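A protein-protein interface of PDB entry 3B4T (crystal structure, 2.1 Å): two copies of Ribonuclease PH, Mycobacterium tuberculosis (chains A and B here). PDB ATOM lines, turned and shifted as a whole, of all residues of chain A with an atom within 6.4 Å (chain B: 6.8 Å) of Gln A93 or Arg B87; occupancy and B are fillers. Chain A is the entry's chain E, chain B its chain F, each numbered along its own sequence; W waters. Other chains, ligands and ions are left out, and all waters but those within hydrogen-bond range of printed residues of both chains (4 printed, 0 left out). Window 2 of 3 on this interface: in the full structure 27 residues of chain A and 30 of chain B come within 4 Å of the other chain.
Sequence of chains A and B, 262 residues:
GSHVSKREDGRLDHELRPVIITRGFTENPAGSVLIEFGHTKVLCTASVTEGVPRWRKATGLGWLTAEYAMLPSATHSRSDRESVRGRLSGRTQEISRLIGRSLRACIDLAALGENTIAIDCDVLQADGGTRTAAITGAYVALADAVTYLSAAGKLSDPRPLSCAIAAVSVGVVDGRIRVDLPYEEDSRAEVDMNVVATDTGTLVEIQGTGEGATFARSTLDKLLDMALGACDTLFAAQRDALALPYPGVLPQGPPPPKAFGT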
ATOM      1  N   TYR A  68      16.869   1.807  16.811  1.00  0.00           N
ATOM      2  CA  TYR A  68      17.814   2.027  17.883  1.00  0.00           C
ATOM      3  C   TYR A  68      19.082   2.630  17.293  1.00  0.00           C
ATOM      4  O   TYR A  68      19.460   2.298  16.167  1.00  0.00           O
ATOM      5  CB  TYR A  68      18.082   0.706  18.605  1.00  0.00           C
ATOM      6  CG  TYR A  68      19.364   0.655  19.436  1.00  0.00           C
ATOM      7  CD1 TYR A  68      19.322   0.687  20.835  1.00  0.00           C
ATOM      8  CD2 TYR A  68      20.615   0.542  18.821  1.00  0.00           C
ATOM      9  CE1 TYR A  68      20.478   0.621  21.576  1.00  0.00           C
ATOM     10  CE2 TYR A  68      21.758   0.482  19.557  1.00  0.00           C
ATOM     11  CZ  TYR A  68      21.683   0.518  20.924  1.00  0.00           C
ATOM     12  OH  TYR A  68      22.834   0.454  21.652  1.00  0.00           O
ATOM     13  N   GLU A  82      26.616   6.822  11.918  1.00  0.00           N
ATOM     14  CA  GLU A  82      26.197   5.924  10.844  1.00  0.00           C
ATOM     15  C   GLU A  82      25.818   6.657   9.561  1.00  0.00           C
ATOM     16  O   GLU A  82      26.109   6.186   8.461  1.00  0.00           O
ATOM     17  CB  GLU A  82      25.046   5.029  11.309  1.00  0.00           C
ATOM     18  CG  GLU A  82      25.498   3.881  12.191  1.00  0.00           C
ATOM     19  CD  GLU A  82      24.350   3.213  12.918  1.00  0.00           C
ATOM     20  OE1 GLU A  82      23.499   3.932  13.483  1.00  0.00           O
ATOM     21  OE2 GLU A  82      24.304   1.967  12.928  1.00  0.00           O
ATOM     22  N   LEU A  88      24.072   1.467   8.023  1.00  0.00           N
ATOM     23  CA  LEU A  88      23.730   1.014   9.365  1.00  0.00           C
ATOM     24  C   LEU A  88      24.600  -0.173   9.757  1.00  0.00           C
ATOM     25  O   LEU A  88      24.795  -1.093   8.961  1.00  0.00           O
ATOM     26  CB  LEU A  88      22.260   0.601   9.426  1.00  0.00           C
ATOM     27  CG  LEU A  88      21.213   1.695   9.235  1.00  0.00           C
ATOM     28  CD1 LEU A  88      19.836   1.081   9.041  1.00  0.00           C
ATOM     29  CD2 LEU A  88      21.220   2.646  10.420  1.00  0.00           C
ATOM     30  N   SER A  89      25.125  -0.158  10.976  1.00  0.00           N
ATOM     31  CA  SER A  89      25.877  -1.305  11.471  1.00  0.00           C
ATOM     32  C   SER A  89      24.916  -2.468  11.684  1.00  0.00           C
ATOM     33  O   SER A  89      23.721  -2.260  11.897  1.00  0.00           O
ATOM     34  CB  SER A  89      26.597  -0.965  12.775  1.00  0.00           C
ATOM     35  OG  SER A  89      25.673  -0.800  13.836  1.00  0.00           O
ATOM     36  N   GLY A  90      25.435  -3.690  11.615  1.00  0.00           N
ATOM     37  CA  GLY A  90      24.610  -4.875  11.775  1.00  0.00           C
ATOM     38  C   GLY A  90      23.966  -4.931  13.145  1.00  0.00           C
ATOM     39  O   GLY A  90      22.806  -5.315  13.291  1.00  0.00           O
ATOM     40  N   ARG A  91      24.734  -4.539  14.154  1.00  0.00           N
ATOM     41  CA  ARG A  91      24.255  -4.506  15.527  1.00  0.00           C
ATOM     42  C   ARG A  91      23.014  -3.621  15.657  1.00  0.00           C
ATOM     43  O   ARG A  91      22.088  -3.941  16.400  1.00  0.00           O
ATOM     44  CB  ARG A  91      25.374  -4.004  16.444  1.00  0.00           C
ATOM     45  CG  ARG A  91      24.922  -3.566  17.821  1.00  0.00           C
ATOM     46  CD  ARG A  91      26.018  -2.765  18.513  1.00  0.00           C
ATOM     47  NE  ARG A  91      25.506  -2.001  19.647  1.00  0.00           N
ATOM     48  CZ  ARG A  91      25.426  -2.475  20.885  1.00  0.00           C
ATOM     49  NH1 ARG A  91      25.830  -3.712  21.145  1.00  0.00           N
ATOM     50  NH2 ARG A  91      24.946  -1.716  21.860  1.00  0.00           N
ATOM     51  N   THR A  92      23.003  -2.516  14.917  1.00  0.00           N
ATOM     52  CA  THR A  92      21.891  -1.570  14.945  1.00  0.00           C
ATOM     53  C   THR A  92      20.585  -2.172  14.436  1.00  0.00           C
ATOM     54  O   THR A  92      19.550  -2.078  15.099  1.00  0.00           O
ATOM     55  CB  THR A  92      22.210  -0.306  14.121  1.00  0.00           C
ATOM     56  OG1 THR A  92      23.207   0.464  14.800  1.00  0.00           O
ATOM     57  CG2 THR A  92      20.962   0.540  13.944  1.00  0.00           C
ATOM     58  N   GLN A  93      20.627  -2.780  13.256  1.00  0.00           N
ATOM     59  CA  GLN A  93      19.425  -3.371  12.674  1.00  0.00           C
ATOM     60  C   GLN A  93      18.929  -4.536  13.524  1.00  0.00           C
ATOM     61  O   GLN A  93      17.726  -4.709  13.725  1.00  0.00           O
ATOM     62  CB  GLN A  93      19.682  -3.827  11.237  1.00  0.00           C
ATOM     63  CG  GLN A  93      20.262  -2.742  10.344  1.00  0.00           C
ATOM     64  CD  GLN A  93      19.967  -2.978   8.879  1.00  0.00           C
ATOM     65  OE1 GLN A  93      20.877  -3.149   8.068  1.00  0.00           O
ATOM     66  NE2 GLN A  93      18.687  -2.994   8.531  1.00  0.00           N
ATOM     67  N   GLU A  94      19.869  -5.328  14.026  1.00  0.00           N
ATOM     68  CA  GLU A  94      19.543  -6.449  14.899  1.00  0.00           C
ATOM     69  C   GLU A  94      18.749  -5.985  16.122  1.00  0.00           C
ATOM     70  O   GLU A  94      17.669  -6.502  16.405  1.00  0.00           O
ATOM     71  CB  GLU A  94      20.827  -7.164  15.323  1.00  0.00           C
ATOM     72  CG  GLU A  94      20.674  -8.134  16.477  1.00  0.00           C
ATOM     73  CD  GLU A  94      22.005  -8.717  16.902  1.00  0.00           C
ATOM     74  OE1 GLU A  94      22.545  -9.566  16.163  1.00  0.00           O
ATOM     75  OE2 GLU A  94      22.518  -8.327  17.971  1.00  0.00           O
ATOM     76  N   ILE A  95      19.281  -4.999  16.837  1.00  0.00           N
ATOM     77  CA  ILE A  95      18.611  -4.468  18.021  1.00  0.00           C
ATOM     78  C   ILE A  95      17.293  -3.771  17.676  1.00  0.00           C
ATOM     79  O   ILE A  95      16.294  -3.941  18.374  1.00  0.00           O
ATOM     80  CB  ILE A  95      19.526  -3.502  18.798  1.00  0.00           C
ATOM     81  CG1 ILE A  95      20.801  -4.228  19.236  1.00  0.00           C
ATOM     82  CG2 ILE A  95      18.796  -2.921  20.003  1.00  0.00           C
ATOM     83  CD1 ILE A  95      21.762  -3.366  20.027  1.00  0.00           C
ATOM     84  N   SER A  96      17.293  -2.990  16.596  1.00  0.00           N
ATOM     85  CA  SER A  96      16.085  -2.296  16.148  1.00  0.00           C
ATOM     86  C   SER A  96      14.925  -3.263  15.921  1.00  0.00           C
ATOM     87  O   SER A  96      13.795  -3.001  16.335  1.00  0.00           O
ATOM     88  CB  SER A  96      16.355  -1.499  14.867  1.00  0.00           C
ATOM     89  OG  SER A  96      17.316  -0.483  15.085  1.00  0.00           O
ATOM     90  N   ARG A  97      15.210  -4.381  15.261  1.00  0.00           N
ATOM     91  CA  ARG A  97      14.190  -5.393  15.003  1.00  0.00           C
ATOM     92  C   ARG A  97      13.674  -6.001  16.304  1.00  0.00           C
ATOM     93  O   ARG A  97      12.466  -6.144  16.494  1.00  0.00           O
ATOM     94  CB  ARG A  97      14.739  -6.484  14.079  1.00  0.00           C
ATOM     95  CG  ARG A  97      15.038  -5.993  12.670  1.00  0.00           C
ATOM     96  CD  ARG A  97      15.871  -6.991  11.887  1.00  0.00           C
ATOM     97  NE  ARG A  97      15.226  -8.299  11.795  1.00  0.00           N
ATOM     98  CZ  ARG A  97      14.301  -8.614  10.893  1.00  0.00           C
ATOM     99  NH1 ARG A  97      13.906  -7.714  10.002  1.00  0.00           N
ATOM    100  NH2 ARG A  97      13.770  -9.829  10.883  1.00  0.00           N
ATOM    101  N   LEU A  98      14.592  -6.352  17.199  1.00  0.00           N
ATOM    102  CA  LEU A  98      14.223  -6.921  18.492  1.00  0.00           C
ATOM    103  C   LEU A  98      13.279  -6.004  19.270  1.00  0.00           C
ATOM    104  O   LEU A  98      12.292  -6.465  19.846  1.00  0.00           O
ATOM    105  CB  LEU A  98      15.468  -7.215  19.328  1.00  0.00           C
ATOM    106  CG  LEU A  98      15.207  -7.647  20.775  1.00  0.00           C
ATOM    107  CD1 LEU A  98      14.478  -8.982  20.822  1.00  0.00           C
ATOM    108  CD2 LEU A  98      16.504  -7.713  21.568  1.00  0.00           C
ATOM    109  N   ARG B  81      16.957  -7.466  -5.029  1.00  0.00           N
ATOM    110  CA  ARG B  81      18.358  -7.748  -4.758  1.00  0.00           C
ATOM    111  C   ARG B  81      18.956  -6.624  -3.916  1.00  0.00           C
ATOM    112  O   ARG B  81      18.818  -5.448  -4.248  1.00  0.00           O
ATOM    113  CB  ARG B  81      19.121  -7.900  -6.077  1.00  0.00           C
ATOM    114  CG  ARG B  81      20.423  -8.672  -5.974  1.00  0.00           C
ATOM    115  CD  ARG B  81      21.126  -8.751  -7.327  1.00  0.00           C
ATOM    116  NE  ARG B  81      20.471  -9.676  -8.248  1.00  0.00           N
ATOM    117  CZ  ARG B  81      20.754 -10.975  -8.320  1.00  0.00           C
ATOM    118  NH1 ARG B  81      21.672 -11.498  -7.519  1.00  0.00           N
ATOM    119  NH2 ARG B  81      20.118 -11.754  -9.183  1.00  0.00           N
ATOM    120  N   GLU B  82      19.617  -6.990  -2.824  1.00  0.00           N
ATOM    121  CA  GLU B  82      20.159  -6.012  -1.882  1.00  0.00           C
ATOM    122  C   GLU B  82      21.229  -5.105  -2.488  1.00  0.00           C
ATOM    123  O   GLU B  82      21.340  -3.932  -2.122  1.00  0.00           O
ATOM    124  CB  GLU B  82      20.710  -6.720  -0.644  1.00  0.00           C
ATOM    125  CG  GLU B  82      19.632  -7.289   0.262  1.00  0.00           C
ATOM    126  CD  GLU B  82      20.187  -8.252   1.288  1.00  0.00           C
ATOM    127  OE1 GLU B  82      20.853  -9.231   0.888  1.00  0.00           O
ATOM    128  OE2 GLU B  82      19.956  -8.029   2.495  1.00  0.00           O
ATOM    129  N   SER B  83      22.025  -5.653  -3.400  1.00  0.00           N
ATOM    130  CA  SER B  83      23.066  -4.876  -4.063  1.00  0.00           C
ATOM    131  C   SER B  83      22.438  -3.786  -4.917  1.00  0.00           C
ATOM    132  O   SER B  83      22.968  -2.681  -5.024  1.00  0.00           O
ATOM    133  CB  SER B  83      23.943  -5.779  -4.933  1.00  0.00           C
ATOM    134  OG  SER B  83      23.179  -6.413  -5.943  1.00  0.00           O
ATOM    135  N   VAL B  84      21.303  -4.108  -5.524  1.00  0.00           N
ATOM    136  CA  VAL B  84      20.582  -3.160  -6.357  1.00  0.00           C
ATOM    137  C   VAL B  84      19.895  -2.115  -5.484  1.00  0.00           C
ATOM    138  O   VAL B  84      19.897  -0.924  -5.801  1.00  0.00           O
ATOM    139  CB  VAL B  84      19.542  -3.877  -7.242  1.00  0.00           C
ATOM    140  CG1 VAL B  84      18.634  -2.870  -7.930  1.00  0.00           C
ATOM    141  CG2 VAL B  84      20.239  -4.764  -8.264  1.00  0.00           C
ATOM    142  N   ARG B  85      19.318  -2.572  -4.378  1.00  0.00           N
ATOM    143  CA  ARG B  85      18.612  -1.696  -3.451  1.00  0.00           C
ATOM    144  C   ARG B  85      19.581  -0.744  -2.748  1.00  0.00           C
ATOM    145  O   ARG B  85      19.192   0.332  -2.295  1.00  0.00           O
ATOM    146  CB  ARG B  85      17.840  -2.531  -2.426  1.00  0.00           C
ATOM    147  CG  ARG B  85      16.489  -1.956  -2.050  1.00  0.00           C
ATOM    148  CD  ARG B  85      15.605  -3.009  -1.405  1.00  0.00           C
ATOM    149  NE  ARG B  85      15.984  -3.276  -0.022  1.00  0.00           N
ATOM    150  CZ  ARG B  85      15.398  -2.718   1.034  1.00  0.00           C
ATOM    151  NH1 ARG B  85      15.806  -3.019   2.260  1.00  0.00           N
ATOM    152  NH2 ARG B  85      14.402  -1.860   0.862  1.00  0.00           N
ATOM    153  N   GLY B  86      20.844  -1.154  -2.659  1.00  0.00           N
ATOM    154  CA  GLY B  86      21.885  -0.316  -2.093  1.00  0.00           C
ATOM    155  C   GLY B  86      22.137  -0.494  -0.604  1.00  0.00           C
ATOM    156  O   GLY B  86      22.936   0.238  -0.017  1.00  0.00           O
ATOM    157  N   ARG B  87      21.466  -1.462   0.014  1.00  0.00           N
ATOM    158  CA  ARG B  87      21.667  -1.720   1.438  1.00  0.00           C
ATOM    159  C   ARG B  87      21.261  -3.136   1.836  1.00  0.00           C
ATOM    160  O   ARG B  87      20.484  -3.792   1.144  1.00  0.00           O
ATOM    161  CB  ARG B  87      20.894  -0.705   2.284  1.00  0.00           C
ATOM    162  CG  ARG B  87      19.391  -0.932   2.301  1.00  0.00           C
ATOM    163  CD  ARG B  87      18.693   0.036   3.244  1.00  0.00           C
ATOM    164  NE  ARG B  87      17.297  -0.332   3.475  1.00  0.00           N
ATOM    165  CZ  ARG B  87      16.881  -1.091   4.485  1.00  0.00           C
ATOM    166  NH1 ARG B  87      17.750  -1.565   5.368  1.00  0.00           N
ATOM    167  NH2 ARG B  87      15.592  -1.377   4.614  1.00  0.00           N
ATOM    168  N   LEU B  88      21.797  -3.598   2.961  1.00  0.00           N
ATOM    169  CA  LEU B  88      21.415  -4.887   3.525  1.00  0.00           C
ATOM    170  C   LEU B  88      20.114  -4.752   4.307  1.00  0.00           C
ATOM    171  O   LEU B  88      19.902  -3.759   5.004  1.00  0.00           O
ATOM    172  CB  LEU B  88      22.516  -5.401   4.450  1.00  0.00           C
ATOM    173  CG  LEU B  88      23.896  -5.589   3.827  1.00  0.00           C
ATOM    174  CD1 LEU B  88      24.954  -5.726   4.912  1.00  0.00           C
ATOM    175  CD2 LEU B  88      23.901  -6.799   2.902  1.00  0.00           C
ATOM    176  N   SER B  89      19.242  -5.747   4.190  1.00  0.00           N
ATOM    177  CA  SER B  89      18.010  -5.768   4.972  1.00  0.00           C
ATOM    178  C   SER B  89      18.308  -6.157   6.417  1.00  0.00           C
ATOM    179  O   SER B  89      19.319  -6.802   6.698  1.00  0.00           O
ATOM    180  CB  SER B  89      16.995  -6.735   4.363  1.00  0.00           C
ATOM    181  OG  SER B  89      17.441  -8.075   4.464  1.00  0.00           O
ATOM    182  N   GLY B  90      17.429  -5.756   7.329  1.00  0.00           N
ATOM    183  CA  GLY B  90      17.604  -6.056   8.738  1.00  0.00           C
ATOM    184  C   GLY B  90      17.686  -7.549   8.992  1.00  0.00           C
ATOM    185  O   GLY B  90      18.491  -8.010   9.799  1.00  0.00           O
ATOM    186  N   ARG B  91      16.846  -8.306   8.296  1.00  0.00           N
ATOM    187  CA  ARG B  91      16.853  -9.759   8.414  1.00  0.00           C
ATOM    188  C   ARG B  91      18.233 -10.328   8.096  1.00  0.00           C
ATOM    189  O   ARG B  91      18.707 -11.249   8.766  1.00  0.00           O
ATOM    190  CB  ARG B  91      15.807 -10.372   7.481  1.00  0.00           C
ATOM    191  CG  ARG B  91      15.863 -11.891   7.399  1.00  0.00           C
ATOM    192  CD  ARG B  91      14.993 -12.410   6.264  1.00  0.00           C
ATOM    193  NE  ARG B  91      15.216 -13.829   6.004  1.00  0.00           N
ATOM    194  CZ  ARG B  91      14.543 -14.809   6.597  1.00  0.00           C
ATOM    195  NH1 ARG B  91      13.604 -14.522   7.488  1.00  0.00           N
ATOM    196  NH2 ARG B  91      14.808 -16.074   6.302  1.00  0.00           N
ATOM    197  N   GLN B  93      21.288  -8.877   8.289  1.00  0.00           N
ATOM    198  CA  GLN B  93      22.297  -8.586   9.302  1.00  0.00           C
ATOM    199  C   GLN B  93      22.075  -9.426  10.554  1.00  0.00           C
ATOM    200  O   GLN B  93      23.025  -9.883  11.187  1.00  0.00           O
ATOM    201  CB  GLN B  93      22.298  -7.097   9.651  1.00  0.00           C
ATOM    202  CG  GLN B  93      23.020  -6.222   8.631  1.00  0.00           C
ATOM    203  CD  GLN B  93      24.533  -6.346   8.720  1.00  0.00           C
ATOM    204  OE1 GLN B  93      25.059  -7.294   9.303  1.00  0.00           O
ATOM    205  NE2 GLN B  93      25.240  -5.380   8.145  1.00  0.00           N
ATOM    206  N   GLU B  94      20.809  -9.622  10.902  1.00  0.00           N
ATOM    207  CA  GLU B  94      20.445 -10.447  12.045  1.00  0.00           C
ATOM    208  C   GLU B  94      20.983 -11.866  11.866  1.00  0.00           C
ATOM    209  O   GLU B  94      21.746 -12.364  12.694  1.00  0.00           O
ATOM    210  CB  GLU B  94      18.926 -10.467  12.196  1.00  0.00           C
ATOM    211  CG  GLU B  94      18.397 -11.433  13.232  1.00  0.00           C
ATOM    212  CD  GLU B  94      16.882 -11.485  13.234  1.00  0.00           C
ATOM    213  OE1 GLU B  94      16.249 -10.408  13.247  1.00  0.00           O
ATOM    214  OE2 GLU B  94      16.322 -12.601  13.223  1.00  0.00           O
HETATM  215  O   HOH W   1      14.298  -7.566   7.078  1.00  0.00           O
HETATM  216  O   HOH W   2      23.415  -3.451   8.560  1.00  0.00           O
HETATM  217  O   HOH W   3      21.228 -11.717  15.333  1.00  0.00           O
HETATM  218  O   HOH W   4      17.432  -9.154  16.080  1.00  0.00           O
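Gly A90 touches Gln B93, and with the chains exchanged Gln A93 touches Gly B90.
Gln A93 touches Leu B88, but with the chains exchanged Leu A88 does not touch Gln B93 (4.4 Å).
Gln A93 touches Ser B89, but with the chains exchanged Ser A89 does not touch Gln B93 (4.6 Å).
Gln B93 touches its own counterpart, Gln A93.
Positions printed for both chains: 82, 88, 89, 90, 91, 93 and 94.
Gln A93 touches just these residues of chain B: Arg B87, Leu B88, Ser B89, Gly B90 and Gln B93.
Arg B87 touches one residue of chain A.
Of the printed residues of chain A, Gly B90 touches Gln A93 and Arg A97.
Of the printed residues of chain A, Glu B94 touches Arg A97 (2.8 Å).
The nearest residue of chain A that does not touch Arg B87 is Leu A88 (5.0 Å).
The nearest printed residue of chain A that does not touch Gln B93 is Leu A88 (4.4 Å).
Of the 13 printed residues of chain B, 7 touch a printed residue of chain A.
Printed residues of chain B that touch a printed residue of chain A: Arg B87, Leu B88, Ser B89, Gly B90, Arg B91, Gln B93 and Glu B94.
Along chain B the printed residues that touch a printed residue of chain A span positions 87 to 94.
Of the 13 printed residues of chain A, 3 touch a printed residue of chain B.
Among the printed residues, Asp or Glu carboxylates within 4 Å of a Lys or Arg side-chain nitrogen of the other chain: Arg A97 with Glu B94 (2.8 Å).
The backbone carbonyl oxygen (O) of Glu B82 is in hydrogen-bond range of the backbone NH (N) of Arg B87 (3.3 Å).
The side-chain carboxylate (OE2) of Glu B82 sits at hydrogen-bond distance from the backbone NH (N) of Ser B89 (2.9 Å).
The side-chain amide nitrogen (NE2) of Gln A93 sits close to the backbone NH (N) of Gly B90 (3.3 Å).
OE1 of Gln A93 sits close to O of Leu B88 (3.3 Å).
The side-chain carboxylate (OE1) of Glu B94 is in salt-bridge range of the guanidinium group (NE) of Arg A97 (2.8 Å).
The guanidinium group (NH1) of Arg A97 sits close to the backbone NH (N) of Arg B91 (3.5 Å).
Gly A90 touches Gln B93.
NH1 of Arg B87 touches NE2 of Gln A93, at 3.6 Å.
NE2 of Gln A93 touches C of Ser B89, 3.8 Å away.
Gln A93 touches Gln B93.
Arg A97 touches Gly B90 (CD to C, 3.5 Å).
Water W2 lies within hydrogen-bond range of the side-chain amide oxygen of Gln A93 (2.6 Å), the side-chain amide nitrogen of Gln B93 (2.7 Å) and the backbone carbonyl oxygen of Leu A88 (2.8 Å).
Water W3 lies within hydrogen-bond range of OE1 of Glu A94 (2.7 Å) and O of Glu B94 (2.8 Å).
Water W4 lies within hydrogen-bond range of the backbone carbonyl oxygen of Glu A94 (2.7 Å) and the side-chain carboxylate of Glu B94 (3.3 Å).
Water W1 bridges the backbone NH of Arg B91 (2.9 Å) and the guanidinium group of Arg A97 (3.0 Å).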
